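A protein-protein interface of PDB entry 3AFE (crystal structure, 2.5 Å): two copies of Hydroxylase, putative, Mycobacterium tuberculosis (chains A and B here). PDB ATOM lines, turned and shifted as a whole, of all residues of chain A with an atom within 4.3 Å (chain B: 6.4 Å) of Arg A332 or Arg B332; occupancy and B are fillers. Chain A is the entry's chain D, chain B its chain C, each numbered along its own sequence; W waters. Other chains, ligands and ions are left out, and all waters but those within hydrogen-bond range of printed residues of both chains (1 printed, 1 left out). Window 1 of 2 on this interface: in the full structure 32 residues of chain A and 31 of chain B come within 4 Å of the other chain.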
ATOM      1  N   ASP A 289      -0.133  12.417  -6.444  1.00  0.00           N
ATOM      2  CA  ASP A 289      -1.257  11.563  -6.789  1.00  0.00           C
ATOM      3  C   ASP A 289      -0.882  10.084  -6.669  1.00  0.00           C
ATOM      4  O   ASP A 289      -1.716   9.261  -6.307  1.00  0.00           O
ATOM      5  CB  ASP A 289      -1.794  11.890  -8.194  1.00  0.00           C
ATOM      6  CG  ASP A 289      -2.385  13.294  -8.287  1.00  0.00           C
ATOM      7  OD1 ASP A 289      -2.669  13.908  -7.237  1.00  0.00           O
ATOM      8  OD2 ASP A 289      -2.562  13.793  -9.418  1.00  0.00           O
ATOM      9  N   ALA A 292      -0.868   9.287  -2.961  1.00  0.00           N
ATOM     10  CA  ALA A 292      -2.252   9.161  -2.508  1.00  0.00           C
ATOM     11  C   ALA A 292      -2.854   7.805  -2.887  1.00  0.00           C
ATOM     12  O   ALA A 292      -3.483   7.159  -2.046  1.00  0.00           O
ATOM     13  CB  ALA A 292      -3.111  10.303  -3.033  1.00  0.00           C
ATOM     14  N   ALA A 293      -2.654   7.373  -4.137  1.00  0.00           N
ATOM     15  CA  ALA A 293      -3.131   6.064  -4.574  1.00  0.00           C
ATOM     16  C   ALA A 293      -2.615   4.971  -3.639  1.00  0.00           C
ATOM     17  O   ALA A 293      -3.392   4.157  -3.128  1.00  0.00           O
ATOM     18  CB  ALA A 293      -2.712   5.775  -6.010  1.00  0.00           C
ATOM     19  N   GLN A 296      -3.997   5.049   0.129  1.00  0.00           N
ATOM     20  CA  GLN A 296      -5.368   4.562   0.228  1.00  0.00           C
ATOM     21  C   GLN A 296      -5.451   3.060  -0.022  1.00  0.00           C
ATOM     22  O   GLN A 296      -6.069   2.323   0.744  1.00  0.00           O
ATOM     23  CB  GLN A 296      -6.285   5.334  -0.726  1.00  0.00           C
ATOM     24  CG  GLN A 296      -6.526   6.747  -0.266  1.00  0.00           C
ATOM     25  CD  GLN A 296      -7.498   7.484  -1.141  1.00  0.00           C
ATOM     26  OE1 GLN A 296      -7.433   7.409  -2.362  1.00  0.00           O
ATOM     27  NE2 GLN A 296      -8.411   8.214  -0.518  1.00  0.00           N
ATOM     28  N   ARG A 328     -10.035   3.834  -7.849  1.00  0.00           N
ATOM     29  CA  ARG A 328      -9.515   5.191  -7.929  1.00  0.00           C
ATOM     30  C   ARG A 328      -7.987   5.157  -7.986  1.00  0.00           C
ATOM     31  O   ARG A 328      -7.367   5.934  -8.706  1.00  0.00           O
ATOM     32  CB  ARG A 328      -9.986   6.018  -6.731  1.00  0.00           C
ATOM     33  CG  ARG A 328      -9.679   7.499  -6.850  1.00  0.00           C
ATOM     34  CD  ARG A 328     -10.606   8.158  -7.863  1.00  0.00           C
ATOM     35  NE  ARG A 328     -10.477   9.614  -7.872  1.00  0.00           N
ATOM     36  CZ  ARG A 328     -11.200  10.410  -8.651  1.00  0.00           C
ATOM     37  NH1 ARG A 328     -12.097   9.883  -9.472  1.00  0.00           N
ATOM     38  NH2 ARG A 328     -11.030  11.727  -8.615  1.00  0.00           N
ATOM     39  N   ALA A 329      -7.388   4.245  -7.226  1.00  0.00           N
ATOM     40  CA  ALA A 329      -5.938   4.125  -7.185  1.00  0.00           C
ATOM     41  C   ALA A 329      -5.415   3.809  -8.569  1.00  0.00           C
ATOM     42  O   ALA A 329      -4.461   4.427  -9.042  1.00  0.00           O
ATOM     43  CB  ALA A 329      -5.502   3.057  -6.182  1.00  0.00           C
ATOM     44  N   THR A 330      -6.039   2.843  -9.227  1.00  0.00           N
ATOM     45  CA  THR A 330      -5.656   2.542 -10.589  1.00  0.00           C
ATOM     46  C   THR A 330      -5.730   3.810 -11.430  1.00  0.00           C
ATOM     47  O   THR A 330      -4.814   4.113 -12.191  1.00  0.00           O
ATOM     48  CB  THR A 330      -6.543   1.470 -11.208  1.00  0.00           C
ATOM     49  OG1 THR A 330      -6.138   0.187 -10.728  1.00  0.00           O
ATOM     50  CG2 THR A 330      -6.406   1.503 -12.717  1.00  0.00           C
ATOM     51  N   GLY A 331      -6.820   4.557 -11.279  1.00  0.00           N
ATOM     52  CA  GLY A 331      -7.029   5.746 -12.080  1.00  0.00           C
ATOM     53  C   GLY A 331      -5.980   6.820 -11.848  1.00  0.00           C
ATOM     54  O   GLY A 331      -5.485   7.429 -12.799  1.00  0.00           O
ATOM     55  N   ARG A 332      -5.641   7.056 -10.582  1.00  0.00           N
ATOM     56  CA  ARG A 332      -4.635   8.055 -10.241  1.00  0.00           C
ATOM     57  C   ARG A 332      -3.320   7.694 -10.886  1.00  0.00           C
ATOM     58  O   ARG A 332      -2.614   8.558 -11.402  1.00  0.00           O
ATOM     59  CB  ARG A 332      -4.433   8.144  -8.727  1.00  0.00           C
ATOM     60  CG  ARG A 332      -5.586   8.781  -7.961  1.00  0.00           C
ATOM     61  CD  ARG A 332      -5.238   8.876  -6.474  1.00  0.00           C
ATOM     62  NE  ARG A 332      -6.423   8.796  -5.629  1.00  0.00           N
ATOM     63  CZ  ARG A 332      -7.205   9.829  -5.360  1.00  0.00           C
ATOM     64  NH1 ARG A 332      -6.922  11.018  -5.878  1.00  0.00           N
ATOM     65  NH2 ARG A 332      -8.272   9.666  -4.587  1.00  0.00           N
ATOM     66  N   SER A 333      -3.002   6.404 -10.835  1.00  0.00           N
ATOM     67  CA  SER A 333      -1.749   5.868 -11.346  1.00  0.00           C
ATOM     68  C   SER A 333      -1.597   6.145 -12.825  1.00  0.00           C
ATOM     69  O   SER A 333      -0.636   6.773 -13.256  1.00  0.00           O
ATOM     70  CB  SER A 333      -1.702   4.358 -11.123  1.00  0.00           C
ATOM     71  OG  SER A 333      -1.439   4.045  -9.769  1.00  0.00           O
ATOM     72  N   ILE A 334      -2.564   5.670 -13.598  1.00  0.00           N
ATOM     73  CA  ILE A 334      -2.536   5.822 -15.039  1.00  0.00           C
ATOM     74  C   ILE A 334      -2.520   7.291 -15.430  1.00  0.00           C
ATOM     75  O   ILE A 334      -1.776   7.689 -16.327  1.00  0.00           O
ATOM     76  CB  ILE A 334      -3.742   5.122 -15.673  1.00  0.00           C
ATOM     77  CG1 ILE A 334      -3.674   3.629 -15.374  1.00  0.00           C
ATOM     78  CG2 ILE A 334      -3.792   5.374 -17.166  1.00  0.00           C
ATOM     79  CD1 ILE A 334      -4.890   2.866 -15.809  1.00  0.00           C
ATOM     80  N   ALA A 335      -3.329   8.101 -14.758  1.00  0.00           N
ATOM     81  CA  ALA A 335      -3.361   9.531 -15.070  1.00  0.00           C
ATOM     82  C   ALA A 335      -1.988  10.141 -14.824  1.00  0.00           C
ATOM     83  O   ALA A 335      -1.522  10.969 -15.615  1.00  0.00           O
ATOM     84  CB  ALA A 335      -4.428  10.261 -14.259  1.00  0.00           C
ATOM     85  N   SER A 336      -1.339   9.717 -13.739  1.00  0.00           N
ATOM     86  CA  SER A 336      -0.001  10.208 -13.404  1.00  0.00           C
ATOM     87  C   SER A 336       1.055   9.732 -14.395  1.00  0.00           C
ATOM     88  O   SER A 336       1.966  10.485 -14.763  1.00  0.00           O
ATOM     89  CB  SER A 336       0.388   9.796 -11.989  1.00  0.00           C
ATOM     90  OG  SER A 336      -0.411  10.486 -11.045  1.00  0.00           O
ATOM     91  N   ALA B 249     -14.815  20.590   2.789  1.00  0.00           N
ATOM     92  CA  ALA B 249     -15.188  19.555   1.828  1.00  0.00           C
ATOM     93  C   ALA B 249     -15.979  18.438   2.508  1.00  0.00           C
ATOM     94  O   ALA B 249     -16.988  17.975   1.975  1.00  0.00           O
ATOM     95  CB  ALA B 249     -13.960  18.994   1.127  1.00  0.00           C
ATOM     96  N   GLU B 285     -16.204   9.466  -6.058  1.00  0.00           N
ATOM     97  CA  GLU B 285     -14.943  10.117  -6.423  1.00  0.00           C
ATOM     98  C   GLU B 285     -14.609  11.222  -5.443  1.00  0.00           C
ATOM     99  O   GLU B 285     -13.477  11.349  -4.996  1.00  0.00           O
ATOM    100  CB  GLU B 285     -15.001  10.704  -7.834  1.00  0.00           C
ATOM    101  CG  GLU B 285     -15.138   9.686  -8.956  1.00  0.00           C
ATOM    102  CD  GLU B 285     -15.148  10.349 -10.321  1.00  0.00           C
ATOM    103  OE1 GLU B 285     -15.711  11.459 -10.428  1.00  0.00           O
ATOM    104  OE2 GLU B 285     -14.595   9.770 -11.284  1.00  0.00           O
ATOM    105  N   ALA B 286     -15.604  12.033  -5.117  1.00  0.00           N
ATOM    106  CA  ALA B 286     -15.406  13.119  -4.172  1.00  0.00           C
ATOM    107  C   ALA B 286     -15.005  12.546  -2.821  1.00  0.00           C
ATOM    108  O   ALA B 286     -14.050  13.019  -2.191  1.00  0.00           O
ATOM    109  CB  ALA B 286     -16.665  13.950  -4.044  1.00  0.00           C
ATOM    110  N   SER B 288     -13.517   9.819  -2.164  1.00  0.00           N
ATOM    111  CA  SER B 288     -12.166   9.273  -2.227  1.00  0.00           C
ATOM    112  C   SER B 288     -11.097  10.360  -2.337  1.00  0.00           C
ATOM    113  O   SER B 288      -9.992  10.209  -1.820  1.00  0.00           O
ATOM    114  CB  SER B 288     -12.044   8.306  -3.400  1.00  0.00           C
ATOM    115  OG  SER B 288     -10.690   7.958  -3.616  1.00  0.00           O
ATOM    116  N   ASP B 289     -11.419  11.453  -3.018  1.00  0.00           N
ATOM    117  CA  ASP B 289     -10.448  12.527  -3.170  1.00  0.00           C
ATOM    118  C   ASP B 289     -10.294  13.289  -1.861  1.00  0.00           C
ATOM    119  O   ASP B 289      -9.201  13.730  -1.515  1.00  0.00           O
ATOM    120  CB  ASP B 289     -10.844  13.481  -4.301  1.00  0.00           C
ATOM    121  CG  ASP B 289     -10.596  12.894  -5.682  1.00  0.00           C
ATOM    122  OD1 ASP B 289     -10.088  11.754  -5.779  1.00  0.00           O
ATOM    123  OD2 ASP B 289     -10.910  13.579  -6.676  1.00  0.00           O
ATOM    124  N   ILE B 290     -11.399  13.445  -1.138  1.00  0.00           N
ATOM    125  CA  ILE B 290     -11.374  14.130   0.146  1.00  0.00           C
ATOM    126  C   ILE B 290     -10.569  13.284   1.137  1.00  0.00           C
ATOM    127  O   ILE B 290      -9.727  13.800   1.898  1.00  0.00           O
ATOM    128  CB  ILE B 290     -12.800  14.378   0.656  1.00  0.00           C
ATOM    129  CG1 ILE B 290     -13.554  15.283  -0.315  1.00  0.00           C
ATOM    130  CG2 ILE B 290     -12.783  15.019   2.027  1.00  0.00           C
ATOM    131  CD1 ILE B 290     -14.987  15.560   0.090  1.00  0.00           C
ATOM    132  N   ALA B 292      -8.233  11.338   0.401  1.00  0.00           N
ATOM    133  CA  ALA B 292      -6.832  11.384   0.009  1.00  0.00           C
ATOM    134  C   ALA B 292      -6.202  12.690   0.470  1.00  0.00           C
ATOM    135  O   ALA B 292      -5.055  12.720   0.937  1.00  0.00           O
ATOM    136  CB  ALA B 292      -6.681  11.206  -1.495  1.00  0.00           C
ATOM    137  N   ALA B 293      -6.960  13.771   0.353  1.00  0.00           N
ATOM    138  CA  ALA B 293      -6.502  15.046   0.880  1.00  0.00           C
ATOM    139  C   ALA B 293      -6.120  14.875   2.348  1.00  0.00           C
ATOM    140  O   ALA B 293      -4.961  15.056   2.714  1.00  0.00           O
ATOM    141  CB  ALA B 293      -7.565  16.110   0.716  1.00  0.00           C
ATOM    142  N   TRP B 294      -7.090  14.489   3.176  1.00  0.00           N
ATOM    143  CA  TRP B 294      -6.851  14.324   4.613  1.00  0.00           C
ATOM    144  C   TRP B 294      -5.690  13.384   4.954  1.00  0.00           C
ATOM    145  O   TRP B 294      -4.787  13.772   5.694  1.00  0.00           O
ATOM    146  CB  TRP B 294      -8.123  13.882   5.349  1.00  0.00           C
ATOM    147  CG  TRP B 294      -7.997  13.969   6.828  1.00  0.00           C
ATOM    148  CD1 TRP B 294      -8.021  12.939   7.715  1.00  0.00           C
ATOM    149  CD2 TRP B 294      -7.807  15.163   7.600  1.00  0.00           C
ATOM    150  NE1 TRP B 294      -7.868  13.412   8.989  1.00  0.00           N
ATOM    151  CE2 TRP B 294      -7.737  14.776   8.947  1.00  0.00           C
ATOM    152  CE3 TRP B 294      -7.696  16.522   7.278  1.00  0.00           C
ATOM    153  CZ2 TRP B 294      -7.558  15.693   9.976  1.00  0.00           C
ATOM    154  CZ3 TRP B 294      -7.527  17.432   8.300  1.00  0.00           C
ATOM    155  CH2 TRP B 294      -7.456  17.016   9.632  1.00  0.00           C
ATOM    156  N   GLN B 296      -3.046  12.484   3.357  1.00  0.00           N
ATOM    157  CA  GLN B 296      -1.760  13.111   3.061  1.00  0.00           C
ATOM    158  C   GLN B 296      -1.442  14.249   4.025  1.00  0.00           C
ATOM    159  O   GLN B 296      -0.374  14.261   4.646  1.00  0.00           O
ATOM    160  CB  GLN B 296      -1.671  13.567   1.592  1.00  0.00           C
ATOM    161  CG  GLN B 296      -1.328  12.421   0.638  1.00  0.00           C
ATOM    162  CD  GLN B 296      -1.183  12.835  -0.822  1.00  0.00           C
ATOM    163  OE1 GLN B 296      -1.917  13.694  -1.324  1.00  0.00           O
ATOM    164  NE2 GLN B 296      -0.240  12.197  -1.521  1.00  0.00           N
ATOM    165  N   ASP B 325       1.989  18.056  -0.882  1.00  0.00           N
ATOM    166  CA  ASP B 325       0.738  17.399  -0.516  1.00  0.00           C
ATOM    167  C   ASP B 325      -0.272  18.416   0.032  1.00  0.00           C
ATOM    168  O   ASP B 325      -1.462  18.342  -0.268  1.00  0.00           O
ATOM    169  CB  ASP B 325       0.981  16.265   0.482  1.00  0.00           C
ATOM    170  CG  ASP B 325       1.567  15.018  -0.177  1.00  0.00           C
ATOM    171  OD1 ASP B 325       1.662  14.988  -1.428  1.00  0.00           O
ATOM    172  OD2 ASP B 325       1.923  14.065   0.556  1.00  0.00           O
ATOM    173  N   VAL B 327      -0.681  21.779  -0.528  1.00  0.00           N
ATOM    174  CA  VAL B 327      -1.328  22.604  -1.536  1.00  0.00           C
ATOM    175  C   VAL B 327      -2.217  21.730  -2.406  1.00  0.00           C
ATOM    176  O   VAL B 327      -3.245  22.166  -2.920  1.00  0.00           O
ATOM    177  CB  VAL B 327      -0.309  23.363  -2.392  1.00  0.00           C
ATOM    178  CG1 VAL B 327       0.479  24.318  -1.518  1.00  0.00           C
ATOM    179  CG2 VAL B 327       0.612  22.395  -3.123  1.00  0.00           C
ATOM    180  N   ARG B 328      -1.824  20.476  -2.540  1.00  0.00           N
ATOM    181  CA  ARG B 328      -2.614  19.529  -3.296  1.00  0.00           C
ATOM    182  C   ARG B 328      -3.920  19.219  -2.561  1.00  0.00           C
ATOM    183  O   ARG B 328      -4.968  19.090  -3.187  1.00  0.00           O
ATOM    184  CB  ARG B 328      -1.806  18.255  -3.547  1.00  0.00           C
ATOM    185  CG  ARG B 328      -1.855  17.791  -4.976  1.00  0.00           C
ATOM    186  CD  ARG B 328      -3.220  17.210  -5.337  1.00  0.00           C
ATOM    187  NE  ARG B 328      -3.454  17.101  -6.781  1.00  0.00           N
ATOM    188  CZ  ARG B 328      -2.504  17.048  -7.713  1.00  0.00           C
ATOM    189  NH1 ARG B 328      -1.224  17.068  -7.372  1.00  0.00           N
ATOM    190  NH2 ARG B 328      -2.835  16.954  -8.997  1.00  0.00           N
ATOM    191  N   ALA B 329      -3.865  19.121  -1.237  1.00  0.00           N
ATOM    192  CA  ALA B 329      -5.059  18.803  -0.454  1.00  0.00           C
ATOM    193  C   ALA B 329      -6.131  19.868  -0.665  1.00  0.00           C
ATOM    194  O   ALA B 329      -7.304  19.570  -0.879  1.00  0.00           O
ATOM    195  CB  ALA B 329      -4.713  18.681   1.031  1.00  0.00           C
ATOM    196  N   THR B 330      -5.712  21.121  -0.608  1.00  0.00           N
ATOM    197  CA  THR B 330      -6.612  22.226  -0.844  1.00  0.00           C
ATOM    198  C   THR B 330      -7.235  22.090  -2.226  1.00  0.00           C
ATOM    199  O   THR B 330      -8.465  22.169  -2.381  1.00  0.00           O
ATOM    200  CB  THR B 330      -5.860  23.544  -0.734  1.00  0.00           C
ATOM    201  OG1 THR B 330      -5.596  23.802   0.650  1.00  0.00           O
ATOM    202  CG2 THR B 330      -6.669  24.693  -1.346  1.00  0.00           C
ATOM    203  N   GLY B 331      -6.383  21.860  -3.222  1.00  0.00           N
ATOM    204  CA  GLY B 331      -6.843  21.701  -4.588  1.00  0.00           C
ATOM    205  C   GLY B 331      -7.968  20.689  -4.714  1.00  0.00           C
ATOM    206  O   GLY B 331      -9.035  21.004  -5.244  1.00  0.00           O
ATOM    207  N   ARG B 332      -7.736  19.474  -4.225  1.00  0.00           N
ATOM    208  CA  ARG B 332      -8.728  18.409  -4.363  1.00  0.00           C
ATOM    209  C   ARG B 332      -9.930  18.538  -3.429  1.00  0.00           C
ATOM    210  O   ARG B 332     -10.974  17.965  -3.693  1.00  0.00           O
ATOM    211  CB  ARG B 332      -8.093  17.022  -4.230  1.00  0.00           C
ATOM    212  CG  ARG B 332      -6.908  16.964  -3.311  1.00  0.00           C
ATOM    213  CD  ARG B 332      -6.546  15.540  -3.031  1.00  0.00           C
ATOM    214  NE  ARG B 332      -6.119  14.874  -4.246  1.00  0.00           N
ATOM    215  CZ  ARG B 332      -4.913  14.346  -4.396  1.00  0.00           C
ATOM    216  NH1 ARG B 332      -4.061  14.407  -3.386  1.00  0.00           N
ATOM    217  NH2 ARG B 332      -4.575  13.752  -5.531  1.00  0.00           N
ATOM    218  N   SER B 333      -9.801  19.295  -2.350  1.00  0.00           N
ATOM    219  CA  SER B 333     -10.969  19.565  -1.521  1.00  0.00           C
ATOM    220  C   SER B 333     -11.889  20.472  -2.329  1.00  0.00           C
ATOM    221  O   SER B 333     -13.088  20.222  -2.456  1.00  0.00           O
ATOM    222  CB  SER B 333     -10.568  20.266  -0.220  1.00  0.00           C
ATOM    223  OG  SER B 333      -9.627  19.503   0.515  1.00  0.00           O
ATOM    224  N   ILE B 334     -11.301  21.521  -2.893  1.00  0.00           N
ATOM    225  CA  ILE B 334     -12.052  22.522  -3.640  1.00  0.00           C
ATOM    226  C   ILE B 334     -12.712  21.937  -4.885  1.00  0.00           C
ATOM    227  O   ILE B 334     -13.897  22.166  -5.128  1.00  0.00           O
ATOM    228  CB  ILE B 334     -11.168  23.737  -3.993  1.00  0.00           C
ATOM    229  CG1 ILE B 334     -10.938  24.580  -2.737  1.00  0.00           C
ATOM    230  CG2 ILE B 334     -11.806  24.577  -5.075  1.00  0.00           C
ATOM    231  CD1 ILE B 334     -10.324  25.918  -3.005  1.00  0.00           C
ATOM    232  N   ALA B 335     -11.948  21.175  -5.659  1.00  0.00           N
ATOM    233  CA  ALA B 335     -12.496  20.481  -6.817  1.00  0.00           C
ATOM    234  C   ALA B 335     -13.672  19.555  -6.437  1.00  0.00           C
ATOM    235  O   ALA B 335     -14.667  19.482  -7.163  1.00  0.00           O
ATOM    236  CB  ALA B 335     -11.400  19.697  -7.535  1.00  0.00           C
ATOM    237  N   SER B 336     -13.558  18.846  -5.312  1.00  0.00           N
ATOM    238  CA  SER B 336     -14.661  18.006  -4.856  1.00  0.00           C
ATOM    239  C   SER B 336     -15.878  18.861  -4.511  1.00  0.00           C
ATOM    240  O   SER B 336     -16.998  18.559  -4.928  1.00  0.00           O
ATOM    241  CB  SER B 336     -14.265  17.154  -3.649  1.00  0.00           C
ATOM    242  OG  SER B 336     -13.247  16.236  -3.986  1.00  0.00           O
ATOM    243  N   ILE B 337     -15.663  19.927  -3.752  1.00  0.00           N
ATOM    244  CA  ILE B 337     -16.773  20.796  -3.396  1.00  0.00           C
ATOM    245  C   ILE B 337     -17.445  21.355  -4.649  1.00  0.00           C
ATOM    246  O   ILE B 337     -18.663  21.434  -4.703  1.00  0.00           O
ATOM    247  CB  ILE B 337     -16.362  21.944  -2.451  1.00  0.00           C
ATOM    248  CG1 ILE B 337     -15.794  21.389  -1.146  1.00  0.00           C
ATOM    249  CG2 ILE B 337     -17.561  22.801  -2.133  1.00  0.00           C
ATOM    250  CD1 ILE B 337     -15.127  22.426  -0.284  1.00  0.00           C
ATOM    251  N   ARG B 339     -17.803  19.927  -7.461  1.00  0.00           N
ATOM    252  CA  ARG B 339     -18.591  18.866  -8.075  1.00  0.00           C
ATOM    253  C   ARG B 339     -19.834  18.531  -7.258  1.00  0.00           C
ATOM    254  O   ARG B 339     -20.889  18.228  -7.811  1.00  0.00           O
ATOM    255  CB  ARG B 339     -17.737  17.625  -8.324  1.00  0.00           C
ATOM    256  CG  ARG B 339     -16.721  17.825  -9.441  1.00  0.00           C
ATOM    257  CD  ARG B 339     -16.149  16.510  -9.913  1.00  0.00           C
ATOM    258  NE  ARG B 339     -14.881  16.695 -10.617  1.00  0.00           N
ATOM    259  CZ  ARG B 339     -13.682  16.418 -10.100  1.00  0.00           C
ATOM    260  NH1 ARG B 339     -12.589  16.632 -10.827  1.00  0.00           N
ATOM    261  NH2 ARG B 339     -13.569  15.922  -8.865  1.00  0.00           N
HETATM  262  O   HOH W   1      -7.895  14.051  -6.470  1.00  0.00           O
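The side-chain carboxylate (OE2) of Glu B285 is in salt-bridge range of the guanidinium group (NH1) of Arg A328, at 3.1 Å. The backbone carbonyl oxygen (O) of Ser B288 sits at hydrogen-bond distance from the side-chain amide nitrogen (NE2) of Gln A296 (2.9 Å). NH2 of Arg A332 is in hydrogen-bond range of OG of Ser B288, 3.1 Å away. The guanidinium group of Arg A328 lies within salt-bridge range of the side-chain carboxylate of Asp B289. NH2 of Arg A332 is in salt-bridge range of OD1 of Asp B289 (3.0 Å). The backbone NH (N) of Ala B292 lies close to the side-chain amide nitrogen (NE2) of Gln A296. The side-chain amide nitrogen (NE2) of Gln B296 sits close to the backbone NH (N) of Ala A292. The side-chain carboxylate (OD2) of Asp A289 lies within salt-bridge range of the guanidinium group (NH2) of Arg B328 (3.2 Å). The side-chain carboxylate (OD1) of Asp A289 lies within salt-bridge range of the guanidinium group (NH2) of Arg B332.
NE2 of Gln B296 lies within hydrogen-bond range of OD1 of Asp B325 (3.4 Å). The guanidinium group (NH1) of Arg B332 is in hydrogen-bond range of the side-chain amide oxygen (OE1) of Gln B296, at 3.1 Å. The side-chain hydroxyl of Ser B336 lies within hydrogen-bond range of the backbone carbonyl oxygen of Arg B332 (2.9 Å). The side-chain amide oxygen (OE1) of Gln A296 is in hydrogen-bond range of the guanidinium group (NH2) of Arg A332, 3.3 Å away. The backbone carbonyl oxygen (O) of Arg A332 is in hydrogen-bond range of the side-chain hydroxyl (OG) of Ser A336 (2.9 Å).
Ala A292 touches Ala B292. Arg A328 touches Ser B288. CB of Ala B292 touches NH2 of Arg A332 (3.8 Å). Arg B332 touches Arg A332.
Of the printed residues of chain B, Arg A332 touches Ser B288 (3.1 Å), Asp B289 (3.0 Å), Ala B292 (3.8 Å) and Arg B332 (3.6 Å). Printed residues of chain B within 4 Å of Gln A296: Ser B288 and Ala B292. Printed residues of chain A within 4 Å of Gln B296: Ala A292 (3.3 Å). Of the printed residues of chain A, Ser B288 touches Gln A296 (2.9 Å), Arg A328 (3.4 Å) and Arg A332 (3.1 Å). Printed residues of chain B within 4 Å of Arg A328: Glu B285, Ser B288 and Asp B289. Of the printed residues of chain A, Ala B292 touches Ala A292 (3.99 Å), Gln A296 (3.3 Å) and Arg A332 (3.8 Å). Ala B293 touches none of the printed residues of chain A. The nearest residue of chain A that does not touch Arg B332 is Ala A292 (4.2 Å). The nearest printed residue of chain A that does not touch Arg B328 is Arg A332 (7.1 Å).
Of the 23 printed residues of chain B, 7 touch a printed residue of chain A. Along chain B the printed residues that touch a printed residue of chain A span positions 285 to 332. Of the 13 printed residues of chain A, 5 touch a printed residue of chain B. Among the printed residues, 13 pairs touch across the chains. Among the printed residues, Asp or Glu carboxylates within 4 Å of a Lys or Arg side-chain nitrogen of the other chain: Asp A289 with Arg B328 (3.2 Å), Asp A289 with Arg B332 (2.6 Å), Arg A328 with Glu B285 (3.1 Å), Arg A328 with Asp B289 (2.7 Å) and Arg A332 with Asp B289 (3.0 Å).
Asp A289 touches Arg B332, and with the chains exchanged Arg A332 touches Asp B289. Ala B292 touches its own counterpart, Ala A292. Ala A292 touches Gln B296, and with the chains exchanged Gln A296 touches Ala B292. Arg A332 touches its own counterpart, Arg B332. 13 positions are printed for both chains.
Water W1 lies within hydrogen-bond range of the guanidinium group (NE) of Arg B332, the side-chain carboxylate (OD2) of Asp B289 and the guanidinium group (NH1) of Arg A332.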
